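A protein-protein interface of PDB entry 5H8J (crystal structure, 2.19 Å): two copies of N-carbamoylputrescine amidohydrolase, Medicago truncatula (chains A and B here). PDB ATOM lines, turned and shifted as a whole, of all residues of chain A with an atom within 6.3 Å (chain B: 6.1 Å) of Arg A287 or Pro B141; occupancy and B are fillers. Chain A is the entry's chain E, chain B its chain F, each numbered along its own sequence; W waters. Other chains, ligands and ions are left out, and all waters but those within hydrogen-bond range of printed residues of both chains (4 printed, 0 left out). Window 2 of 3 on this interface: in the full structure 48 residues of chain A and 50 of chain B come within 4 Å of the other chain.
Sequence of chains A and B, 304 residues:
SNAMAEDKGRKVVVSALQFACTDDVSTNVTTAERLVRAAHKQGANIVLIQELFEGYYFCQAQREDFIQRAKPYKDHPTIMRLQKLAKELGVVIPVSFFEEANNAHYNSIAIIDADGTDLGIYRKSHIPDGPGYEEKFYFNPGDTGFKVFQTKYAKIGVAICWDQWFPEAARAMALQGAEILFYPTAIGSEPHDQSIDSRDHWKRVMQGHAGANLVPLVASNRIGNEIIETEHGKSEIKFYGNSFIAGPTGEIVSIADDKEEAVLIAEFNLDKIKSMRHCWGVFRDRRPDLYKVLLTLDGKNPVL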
ATOM      1  N   ASP A 285     -29.147   3.095 -25.532  1.00  0.00           N
ATOM      2  CA  ASP A 285     -27.714   2.908 -25.800  1.00  0.00           C
ATOM      3  C   ASP A 285     -26.810   4.080 -25.388  1.00  0.00           C
ATOM      4  O   ASP A 285     -25.612   3.993 -25.556  1.00  0.00           O
ATOM      5  CB  ASP A 285     -27.512   2.574 -27.320  1.00  0.00           C
ATOM      6  CG  ASP A 285     -28.306   1.357 -27.774  1.00  0.00           C
ATOM      7  OD1 ASP A 285     -28.744   0.605 -26.918  1.00  0.00           O
ATOM      8  OD2 ASP A 285     -28.471   1.152 -29.002  1.00  0.00           O
ATOM      9  N   ARG A 286     -27.384   5.157 -24.857  1.00  0.00           N
ATOM     10  CA  ARG A 286     -26.616   6.297 -24.425  1.00  0.00           C
ATOM     11  C   ARG A 286     -25.665   5.882 -23.311  1.00  0.00           C
ATOM     12  O   ARG A 286     -25.932   4.969 -22.555  1.00  0.00           O
ATOM     13  CB  ARG A 286     -27.517   7.449 -23.977  1.00  0.00           C
ATOM     14  CG  ARG A 286     -28.238   8.131 -25.129  1.00  0.00           C
ATOM     15  CD  ARG A 286     -29.101   9.290 -24.704  1.00  0.00           C
ATOM     16  NE  ARG A 286     -28.315  10.401 -24.151  1.00  0.00           N
ATOM     17  CZ  ARG A 286     -28.176  10.661 -22.837  1.00  0.00           C
ATOM     18  NH1 ARG A 286     -28.785   9.901 -21.936  1.00  0.00           N
ATOM     19  NH2 ARG A 286     -27.434  11.700 -22.436  1.00  0.00           N
ATOM     20  N   ARG A 287     -24.542   6.586 -23.246  1.00  0.00           N
ATOM     21  CA  ARG A 287     -23.455   6.333 -22.315  1.00  0.00           C
ATOM     22  C   ARG A 287     -23.173   7.564 -21.442  1.00  0.00           C
ATOM     23  O   ARG A 287     -22.102   8.180 -21.563  1.00  0.00           O
ATOM     24  CB  ARG A 287     -22.200   6.001 -23.125  1.00  0.00           C
ATOM     25  CG  ARG A 287     -22.279   4.723 -23.936  1.00  0.00           C
ATOM     26  CD  ARG A 287     -22.329   3.485 -23.053  1.00  0.00           C
ATOM     27  NE  ARG A 287     -21.282   3.479 -22.032  1.00  0.00           N
ATOM     28  CZ  ARG A 287     -20.024   3.041 -22.228  1.00  0.00           C
ATOM     29  NH1 ARG A 287     -19.657   2.579 -23.412  1.00  0.00           N
ATOM     30  NH2 ARG A 287     -19.147   3.083 -21.240  1.00  0.00           N
ATOM     31  N   PRO A 288     -24.138   7.938 -20.555  1.00  0.00           N
ATOM     32  CA  PRO A 288     -23.905   9.111 -19.690  1.00  0.00           C
ATOM     33  C   PRO A 288     -22.583   9.002 -18.880  1.00  0.00           C
ATOM     34  O   PRO A 288     -21.986  10.044 -18.540  1.00  0.00           O
ATOM     35  CB  PRO A 288     -25.129   9.153 -18.779  1.00  0.00           C
ATOM     36  CG  PRO A 288     -25.742   7.736 -18.877  1.00  0.00           C
ATOM     37  CD  PRO A 288     -25.418   7.281 -20.267  1.00  0.00           C
ATOM     38  N   ASP A 289     -22.124   7.788 -18.586  1.00  0.00           N
ATOM     39  CA  ASP A 289     -20.842   7.635 -17.921  1.00  0.00           C
ATOM     40  C   ASP A 289     -19.622   8.208 -18.734  1.00  0.00           C
ATOM     41  O   ASP A 289     -18.539   8.400 -18.169  1.00  0.00           O
ATOM     42  CB  ASP A 289     -20.558   6.188 -17.514  1.00  0.00           C
ATOM     43  CG  ASP A 289     -20.678   5.161 -18.679  1.00  0.00           C
ATOM     44  OD1 ASP A 289     -21.523   5.330 -19.570  1.00  0.00           O
ATOM     45  OD2 ASP A 289     -19.953   4.196 -18.669  1.00  0.00           O
ATOM     46  N   LEU A 290     -19.796   8.476 -20.023  1.00  0.00           N
ATOM     47  CA  LEU A 290     -18.694   8.922 -20.847  1.00  0.00           C
ATOM     48  C   LEU A 290     -18.932  10.325 -21.340  1.00  0.00           C
ATOM     49  O   LEU A 290     -18.190  10.788 -22.199  1.00  0.00           O
ATOM     50  CB  LEU A 290     -18.551   8.007 -22.068  1.00  0.00           C
ATOM     51  CG  LEU A 290     -18.281   6.536 -21.867  1.00  0.00           C
ATOM     52  CD1 LEU A 290     -18.293   5.797 -23.209  1.00  0.00           C
ATOM     53  CD2 LEU A 290     -16.946   6.333 -21.162  1.00  0.00           C
ATOM     54  N   TYR A 291     -19.979  10.991 -20.826  1.00  0.00           N
ATOM     55  CA  TYR A 291     -20.348  12.345 -21.279  1.00  0.00           C
ATOM     56  C   TYR A 291     -19.902  13.486 -20.331  1.00  0.00           C
ATOM     57  O   TYR A 291     -20.357  14.587 -20.483  1.00  0.00           O
ATOM     58  CB  TYR A 291     -21.855  12.465 -21.476  1.00  0.00           C
ATOM     59  CG  TYR A 291     -22.469  11.495 -22.458  1.00  0.00           C
ATOM     60  CD1 TYR A 291     -21.715  10.870 -23.473  1.00  0.00           C
ATOM     61  CD2 TYR A 291     -23.831  11.227 -22.410  1.00  0.00           C
ATOM     62  CE1 TYR A 291     -22.313   9.990 -24.360  1.00  0.00           C
ATOM     63  CE2 TYR A 291     -24.423  10.344 -23.301  1.00  0.00           C
ATOM     64  CZ  TYR A 291     -23.676   9.731 -24.271  1.00  0.00           C
ATOM     65  OH  TYR A 291     -24.331   8.874 -25.123  1.00  0.00           O
ATOM     66  N   LYS A 292     -19.035  13.202 -19.373  1.00  0.00           N
ATOM     67  CA  LYS A 292     -18.625  14.225 -18.398  1.00  0.00           C
ATOM     68  C   LYS A 292     -18.023  15.461 -19.044  1.00  0.00           C
ATOM     69  O   LYS A 292     -18.257  16.517 -18.581  1.00  0.00           O
ATOM     70  CB  LYS A 292     -17.680  13.697 -17.332  1.00  0.00           C
ATOM     71  CG  LYS A 292     -18.367  12.875 -16.236  1.00  0.00           C
ATOM     72  CD  LYS A 292     -17.311  12.366 -15.228  1.00  0.00           C
ATOM     73  CE  LYS A 292     -17.812  11.144 -14.421  1.00  0.00           C
ATOM     74  NZ  LYS A 292     -19.172  11.418 -13.833  1.00  0.00           N
ATOM     75  N   HIS B 105     -14.114  -7.924 -25.103  1.00  0.00           N
ATOM     76  CA  HIS B 105     -14.046  -7.815 -26.562  1.00  0.00           C
ATOM     77  C   HIS B 105     -14.631  -6.489 -26.949  1.00  0.00           C
ATOM     78  O   HIS B 105     -15.572  -6.060 -26.344  1.00  0.00           O
ATOM     79  CB  HIS B 105     -14.823  -8.909 -27.259  1.00  0.00           C
ATOM     80  CG  HIS B 105     -14.299 -10.274 -26.997  1.00  0.00           C
ATOM     81  ND1 HIS B 105     -14.549 -10.940 -25.826  1.00  0.00           N
ATOM     82  CD2 HIS B 105     -13.538 -11.104 -27.751  1.00  0.00           C
ATOM     83  CE1 HIS B 105     -13.971 -12.129 -25.861  1.00  0.00           C
ATOM     84  NE2 HIS B 105     -13.351 -12.254 -27.022  1.00  0.00           N
ATOM     85  N   TYR B 106     -14.073  -5.857 -27.973  1.00  0.00           N
ATOM     86  CA  TYR B 106     -14.492  -4.539 -28.397  1.00  0.00           C
ATOM     87  C   TYR B 106     -14.510  -4.368 -29.890  1.00  0.00           C
ATOM     88  O   TYR B 106     -13.880  -5.104 -30.616  1.00  0.00           O
ATOM     89  CB  TYR B 106     -13.483  -3.514 -27.884  1.00  0.00           C
ATOM     90  CG  TYR B 106     -13.252  -3.497 -26.410  1.00  0.00           C
ATOM     91  CD1 TYR B 106     -14.086  -2.809 -25.584  1.00  0.00           C
ATOM     92  CD2 TYR B 106     -12.173  -4.164 -25.840  1.00  0.00           C
ATOM     93  CE1 TYR B 106     -13.878  -2.779 -24.199  1.00  0.00           C
ATOM     94  CE2 TYR B 106     -11.950  -4.137 -24.463  1.00  0.00           C
ATOM     95  CZ  TYR B 106     -12.810  -3.439 -23.657  1.00  0.00           C
ATOM     96  OH  TYR B 106     -12.629  -3.385 -22.315  1.00  0.00           O
ATOM     97  N   ARG B 123     -12.407   2.675 -28.578  1.00  0.00           N
ATOM     98  CA  ARG B 123     -13.293   1.541 -28.457  1.00  0.00           C
ATOM     99  C   ARG B 123     -14.748   2.050 -28.589  1.00  0.00           C
ATOM    100  O   ARG B 123     -15.168   2.930 -27.837  1.00  0.00           O
ATOM    101  CB  ARG B 123     -13.061   0.864 -27.121  1.00  0.00           C
ATOM    102  CG  ARG B 123     -11.712   0.131 -27.064  1.00  0.00           C
ATOM    103  CD  ARG B 123     -11.400  -0.470 -25.687  1.00  0.00           C
ATOM    104  NE  ARG B 123     -10.303  -1.419 -25.719  1.00  0.00           N
ATOM    105  CZ  ARG B 123      -9.722  -1.920 -24.642  1.00  0.00           C
ATOM    106  NH1 ARG B 123     -10.128  -1.547 -23.423  1.00  0.00           N
ATOM    107  NH2 ARG B 123      -8.741  -2.780 -24.766  1.00  0.00           N
ATOM    108  N   LYS B 124     -15.495   1.503 -29.544  1.00  0.00           N
ATOM    109  CA  LYS B 124     -16.909   1.894 -29.798  1.00  0.00           C
ATOM    110  C   LYS B 124     -17.678   1.982 -28.485  1.00  0.00           C
ATOM    111  O   LYS B 124     -17.671   1.018 -27.718  1.00  0.00           O
ATOM    112  CB  LYS B 124     -17.564   0.861 -30.719  1.00  0.00           C
ATOM    113  CG  LYS B 124     -18.931   1.235 -31.207  1.00  0.00           C
ATOM    114  CD  LYS B 124     -19.333   0.273 -32.288  1.00  0.00           C
ATOM    115  CE  LYS B 124     -20.697   0.628 -32.823  1.00  0.00           C
ATOM    116  NZ  LYS B 124     -21.015  -0.186 -34.037  1.00  0.00           N
ATOM    117  N   SER B 125     -18.325   3.130 -28.226  1.00  0.00           N
ATOM    118  CA  SER B 125     -19.032   3.344 -26.956  1.00  0.00           C
ATOM    119  C   SER B 125     -20.495   2.932 -26.958  1.00  0.00           C
ATOM    120  O   SER B 125     -20.980   2.352 -25.977  1.00  0.00           O
ATOM    121  CB  SER B 125     -18.971   4.842 -26.568  1.00  0.00           C
ATOM    122  OG  SER B 125     -17.647   5.319 -26.542  1.00  0.00           O
ATOM    123  N   HIS B 126     -21.196   3.247 -28.040  1.00  0.00           N
ATOM    124  CA  HIS B 126     -22.621   2.941 -28.145  1.00  0.00           C
ATOM    125  C   HIS B 126     -22.771   1.653 -28.957  1.00  0.00           C
ATOM    126  O   HIS B 126     -22.354   1.617 -30.107  1.00  0.00           O
ATOM    127  CB  HIS B 126     -23.374   4.104 -28.823  1.00  0.00           C
ATOM    128  CG  HIS B 126     -23.090   5.435 -28.215  1.00  0.00           C
ATOM    129  ND1 HIS B 126     -22.085   6.254 -28.676  1.00  0.00           N
ATOM    130  CD2 HIS B 126     -23.657   6.092 -27.170  1.00  0.00           C
ATOM    131  CE1 HIS B 126     -22.042   7.361 -27.952  1.00  0.00           C
ATOM    132  NE2 HIS B 126     -22.986   7.293 -27.031  1.00  0.00           N
ATOM    133  N   ILE B 127     -23.365   0.613 -28.375  1.00  0.00           N
ATOM    134  CA  ILE B 127     -23.448  -0.704 -29.059  1.00  0.00           C
ATOM    135  C   ILE B 127     -24.904  -1.022 -29.533  1.00  0.00           C
ATOM    136  O   ILE B 127     -25.826  -1.149 -28.708  1.00  0.00           O
ATOM    137  CB  ILE B 127     -22.950  -1.853 -28.163  1.00  0.00           C
ATOM    138  CG1 ILE B 127     -21.618  -1.507 -27.462  1.00  0.00           C
ATOM    139  CG2 ILE B 127     -22.858  -3.162 -28.955  1.00  0.00           C
ATOM    140  CD1 ILE B 127     -20.476  -1.288 -28.422  1.00  0.00           C
ATOM    141  N   PHE B 139     -19.491  -7.294 -28.394  1.00  0.00           N
ATOM    142  CA  PHE B 139     -18.629  -6.246 -27.893  1.00  0.00           C
ATOM    143  C   PHE B 139     -19.053  -5.650 -26.578  1.00  0.00           C
ATOM    144  O   PHE B 139     -20.204  -5.228 -26.415  1.00  0.00           O
ATOM    145  CB  PHE B 139     -18.620  -5.068 -28.867  1.00  0.00           C
ATOM    146  CG  PHE B 139     -18.495  -5.440 -30.330  1.00  0.00           C
ATOM    147  CD1 PHE B 139     -17.420  -6.162 -30.798  1.00  0.00           C
ATOM    148  CD2 PHE B 139     -19.476  -5.017 -31.247  1.00  0.00           C
ATOM    149  CE1 PHE B 139     -17.324  -6.489 -32.156  1.00  0.00           C
ATOM    150  CE2 PHE B 139     -19.389  -5.336 -32.599  1.00  0.00           C
ATOM    151  CZ  PHE B 139     -18.313  -6.069 -33.053  1.00  0.00           C
ATOM    152  N   ASN B 140     -18.118  -5.598 -25.636  1.00  0.00           N
ATOM    153  CA  ASN B 140     -18.342  -4.860 -24.418  1.00  0.00           C
ATOM    154  C   ASN B 140     -18.501  -3.419 -24.861  1.00  0.00           C
ATOM    155  O   ASN B 140     -17.904  -3.002 -25.865  1.00  0.00           O
ATOM    156  CB  ASN B 140     -17.132  -4.882 -23.462  1.00  0.00           C
ATOM    157  CG  ASN B 140     -16.912  -6.215 -22.792  1.00  0.00           C
ATOM    158  OD1 ASN B 140     -16.500  -7.190 -23.417  1.00  0.00           O
ATOM    159  ND2 ASN B 140     -17.155  -6.247 -21.478  1.00  0.00           N
ATOM    160  N   PRO B 141     -19.321  -2.660 -24.134  1.00  0.00           N
ATOM    161  CA  PRO B 141     -19.391  -1.231 -24.399  1.00  0.00           C
ATOM    162  C   PRO B 141     -18.000  -0.597 -24.111  1.00  0.00           C
ATOM    163  O   PRO B 141     -17.406  -0.867 -23.061  1.00  0.00           O
ATOM    164  CB  PRO B 141     -20.481  -0.728 -23.421  1.00  0.00           C
ATOM    165  CG  PRO B 141     -21.281  -1.979 -23.055  1.00  0.00           C
ATOM    166  CD  PRO B 141     -20.288  -3.101 -23.093  1.00  0.00           C
ATOM    167  N   GLY B 142     -17.510   0.212 -25.057  1.00  0.00           N
ATOM    168  CA  GLY B 142     -16.190   0.853 -24.984  1.00  0.00           C
ATOM    169  C   GLY B 142     -15.908   1.581 -23.677  1.00  0.00           C
ATOM    170  O   GLY B 142     -16.806   2.202 -23.093  1.00  0.00           O
ATOM    171  N   ASP B 143     -14.646   1.495 -23.245  1.00  0.00           N
ATOM    172  CA  ASP B 143     -14.187   2.098 -22.000  1.00  0.00           C
ATOM    173  C   ASP B 143     -13.047   3.082 -22.151  1.00  0.00           C
ATOM    174  O   ASP B 143     -12.459   3.474 -21.164  1.00  0.00           O
ATOM    175  CB  ASP B 143     -13.809   1.021 -20.985  1.00  0.00           C
ATOM    176  CG  ASP B 143     -12.860  -0.011 -21.539  1.00  0.00           C
ATOM    177  OD1 ASP B 143     -12.268   0.219 -22.617  1.00  0.00           O
ATOM    178  OD2 ASP B 143     -12.716  -1.080 -20.897  1.00  0.00           O
ATOM    179  N   PHE B 146     -14.592   9.117 -25.450  1.00  0.00           N
ATOM    180  CA  PHE B 146     -14.381   9.792 -26.758  1.00  0.00           C
ATOM    181  C   PHE B 146     -13.027  10.453 -26.793  1.00  0.00           C
ATOM    182  O   PHE B 146     -12.610  11.091 -25.803  1.00  0.00           O
ATOM    183  CB  PHE B 146     -15.553  10.723 -27.048  1.00  0.00           C
ATOM    184  CG  PHE B 146     -16.839  10.007 -26.874  1.00  0.00           C
ATOM    185  CD1 PHE B 146     -17.202   9.034 -27.777  1.00  0.00           C
ATOM    186  CD2 PHE B 146     -17.640  10.244 -25.771  1.00  0.00           C
ATOM    187  CE1 PHE B 146     -18.366   8.311 -27.621  1.00  0.00           C
ATOM    188  CE2 PHE B 146     -18.819   9.530 -25.597  1.00  0.00           C
ATOM    189  CZ  PHE B 146     -19.179   8.560 -26.523  1.00  0.00           C
ATOM    190  N   PHE B 166     -25.265   9.767 -32.157  1.00  0.00           N
ATOM    191  CA  PHE B 166     -25.264  10.462 -30.862  1.00  0.00           C
ATOM    192  C   PHE B 166     -24.540  11.832 -30.892  1.00  0.00           C
ATOM    193  O   PHE B 166     -23.285  11.908 -31.015  1.00  0.00           O
ATOM    194  CB  PHE B 166     -24.646   9.557 -29.771  1.00  0.00           C
ATOM    195  CG  PHE B 166     -25.371   8.239 -29.593  1.00  0.00           C
ATOM    196  CD1 PHE B 166     -25.123   7.179 -30.438  1.00  0.00           C
ATOM    197  CD2 PHE B 166     -26.318   8.077 -28.577  1.00  0.00           C
ATOM    198  CE1 PHE B 166     -25.806   5.956 -30.279  1.00  0.00           C
ATOM    199  CE2 PHE B 166     -26.995   6.875 -28.414  1.00  0.00           C
ATOM    200  CZ  PHE B 166     -26.739   5.812 -29.267  1.00  0.00           C
ATOM    201  N   LEU B 294     -27.933  15.476 -18.910  1.00  0.00           N
ATOM    202  CA  LEU B 294     -27.324  14.606 -19.928  1.00  0.00           C
ATOM    203  C   LEU B 294     -26.544  13.436 -19.272  1.00  0.00           C
ATOM    204  O   LEU B 294     -26.148  12.497 -19.952  1.00  0.00           O
ATOM    205  CB  LEU B 294     -26.426  15.351 -20.896  1.00  0.00           C
ATOM    206  CG  LEU B 294     -26.991  16.591 -21.610  1.00  0.00           C
ATOM    207  CD1 LEU B 294     -25.961  17.190 -22.572  1.00  0.00           C
ATOM    208  CD2 LEU B 294     -28.298  16.283 -22.321  1.00  0.00           C
ATOM    209  N   LEU B 297     -29.994   8.656 -17.726  1.00  0.00           N
ATOM    210  CA  LEU B 297     -30.578   7.895 -18.811  1.00  0.00           C
ATOM    211  C   LEU B 297     -32.084   8.187 -18.891  1.00  0.00           C
ATOM    212  O   LEU B 297     -32.645   8.238 -19.988  1.00  0.00           O
ATOM    213  CB  LEU B 297     -30.384   6.390 -18.582  1.00  0.00           C
ATOM    214  CG  LEU B 297     -29.014   5.747 -18.837  1.00  0.00           C
ATOM    215  CD1 LEU B 297     -29.022   4.261 -18.384  1.00  0.00           C
ATOM    216  CD2 LEU B 297     -28.650   5.881 -20.310  1.00  0.00           C
HETATM  217  O   HOH W   1     -17.686   0.320 -20.335  1.00  0.00           O
HETATM  218  O   HOH W   2     -24.513   1.290 -25.816  1.00  0.00           O
HETATM  219  O   HOH W   3     -30.991   7.756 -22.231  1.00  0.00           O
HETATM  220  O   HOH W   4     -15.640  10.144 -22.740  1.00  0.00           O
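The guanidinium group of Arg A286 is in hydrogen-bond range of the backbone carbonyl oxygen of Leu B294 (2.9 Å). O of Ser B125 lies within hydrogen-bond range of NH1 of Arg A287 (2.9 Å). The guanidinium group (NH1) of Arg A287 sits at hydrogen-bond distance from the backbone carbonyl oxygen (O) of Gly B142, 2.9 Å away. The side-chain hydroxyl (OH) of Tyr A291 lies within hydrogen-bond range of a ring nitrogen (NE2) of His B126, 2.8 Å away.
Among the printed residues, pairs that only touch across the chains: Asp A285 with His B126, Asp A285 with Ile B127, Asp A285 with Phe B166, Arg A286 with Phe B166, Arg A286 with Leu B297, Arg A287 with His B126, Arg A287 with Pro B141, Pro A288 with Leu B294, Pro A288 with Leu B297, Leu A290 with Ser B125, Leu A290 with Gly B142, Leu A290 with Phe B146, Tyr A291 with Phe B146 and Tyr A291 with Leu B294.
No position is printed for both chains. Of the 18 pairs that touch across the chains among the printed residues, none has its exchanged pair printed and touching as well.
NH2 of Arg A287 is in salt-bridge range of OD2 of Asp A289 (2.9 Å). The backbone NH (N) of Arg A287 sits at hydrogen-bond distance from the side-chain hydroxyl (OH) of Tyr A291, at 3.0 Å. N of Gly B142 sits at hydrogen-bond distance from O of Lys B124 (2.8 Å).
Water W4 bridges the backbone carbonyl oxygen (O) of Leu A290 and the backbone NH (N) of Phe B146. Water W3 lies within hydrogen-bond range of O of Leu B297 (2.8 Å) and NH1 of Arg A286 (3.1 Å). Water W2 lies within hydrogen-bond range of N of Ile B127 (2.9 Å) and O of Asp A285 (2.9 Å). Water W1 lies within hydrogen-bond range of the backbone carbonyl oxygen (O) of Pro B141 (3.0 Å), the guanidinium group (NH2) of Arg A287 (3.3 Å) and the backbone carbonyl oxygen (O) of Gly B142 (3.5 Å).
Of the 16 printed residues of chain B, 9 touch a printed residue of chain A. Printed residues of chain B that touch a printed residue of chain A: Ser B125, His B126, Ile B127, Pro B141, Gly B142, Phe B146, Phe B166, Leu B294 and Leu B297. Of the 8 printed residues of chain A, 6 touch a printed residue of chain B. Hydrophobic or aromatic side chains of chain A within 4 Å of the printed part of chain B: Pro A288, Leu A290 and Tyr A291. Among the printed residues, 18 pairs touch across the chains. Among the printed residues, no Asp or Glu carboxylate lies within 4 Å of a Lys or Arg side-chain nitrogen of the other chain.
Printed residues of chain B within 4 Å of Arg A286: Phe B166, Leu B294 and Leu B297. Of the printed residues of chain B, Arg A287 touches Ser B125 (2.9 Å), His B126 (3.8 Å), Pro B141 (3.4 Å) and Gly B142 (2.9 Å). Printed residues of chain B within 4 Å of Pro A288: Leu B294 (3.7 Å) and Leu B297 (3.5 Å). Of the printed residues of chain B, Leu A290 touches Ser B125, Gly B142 and Phe B146. Lys A292 touches none of the printed residues of chain B. Lys B124 touches none of the printed residues of chain A. Of the printed residues of chain A, Pro B141 touches Arg A287. Printed residues of chain A within 4 Å of Phe B166: Asp A285 (3.9 Å) and Arg A286 (3.7 Å). Printed residues of chain A within 4 Å of Leu B297: Arg A286 and Pro A288. The nearest residue of chain B that does not touch Arg A287 is Lys B124 (5.0 Å).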
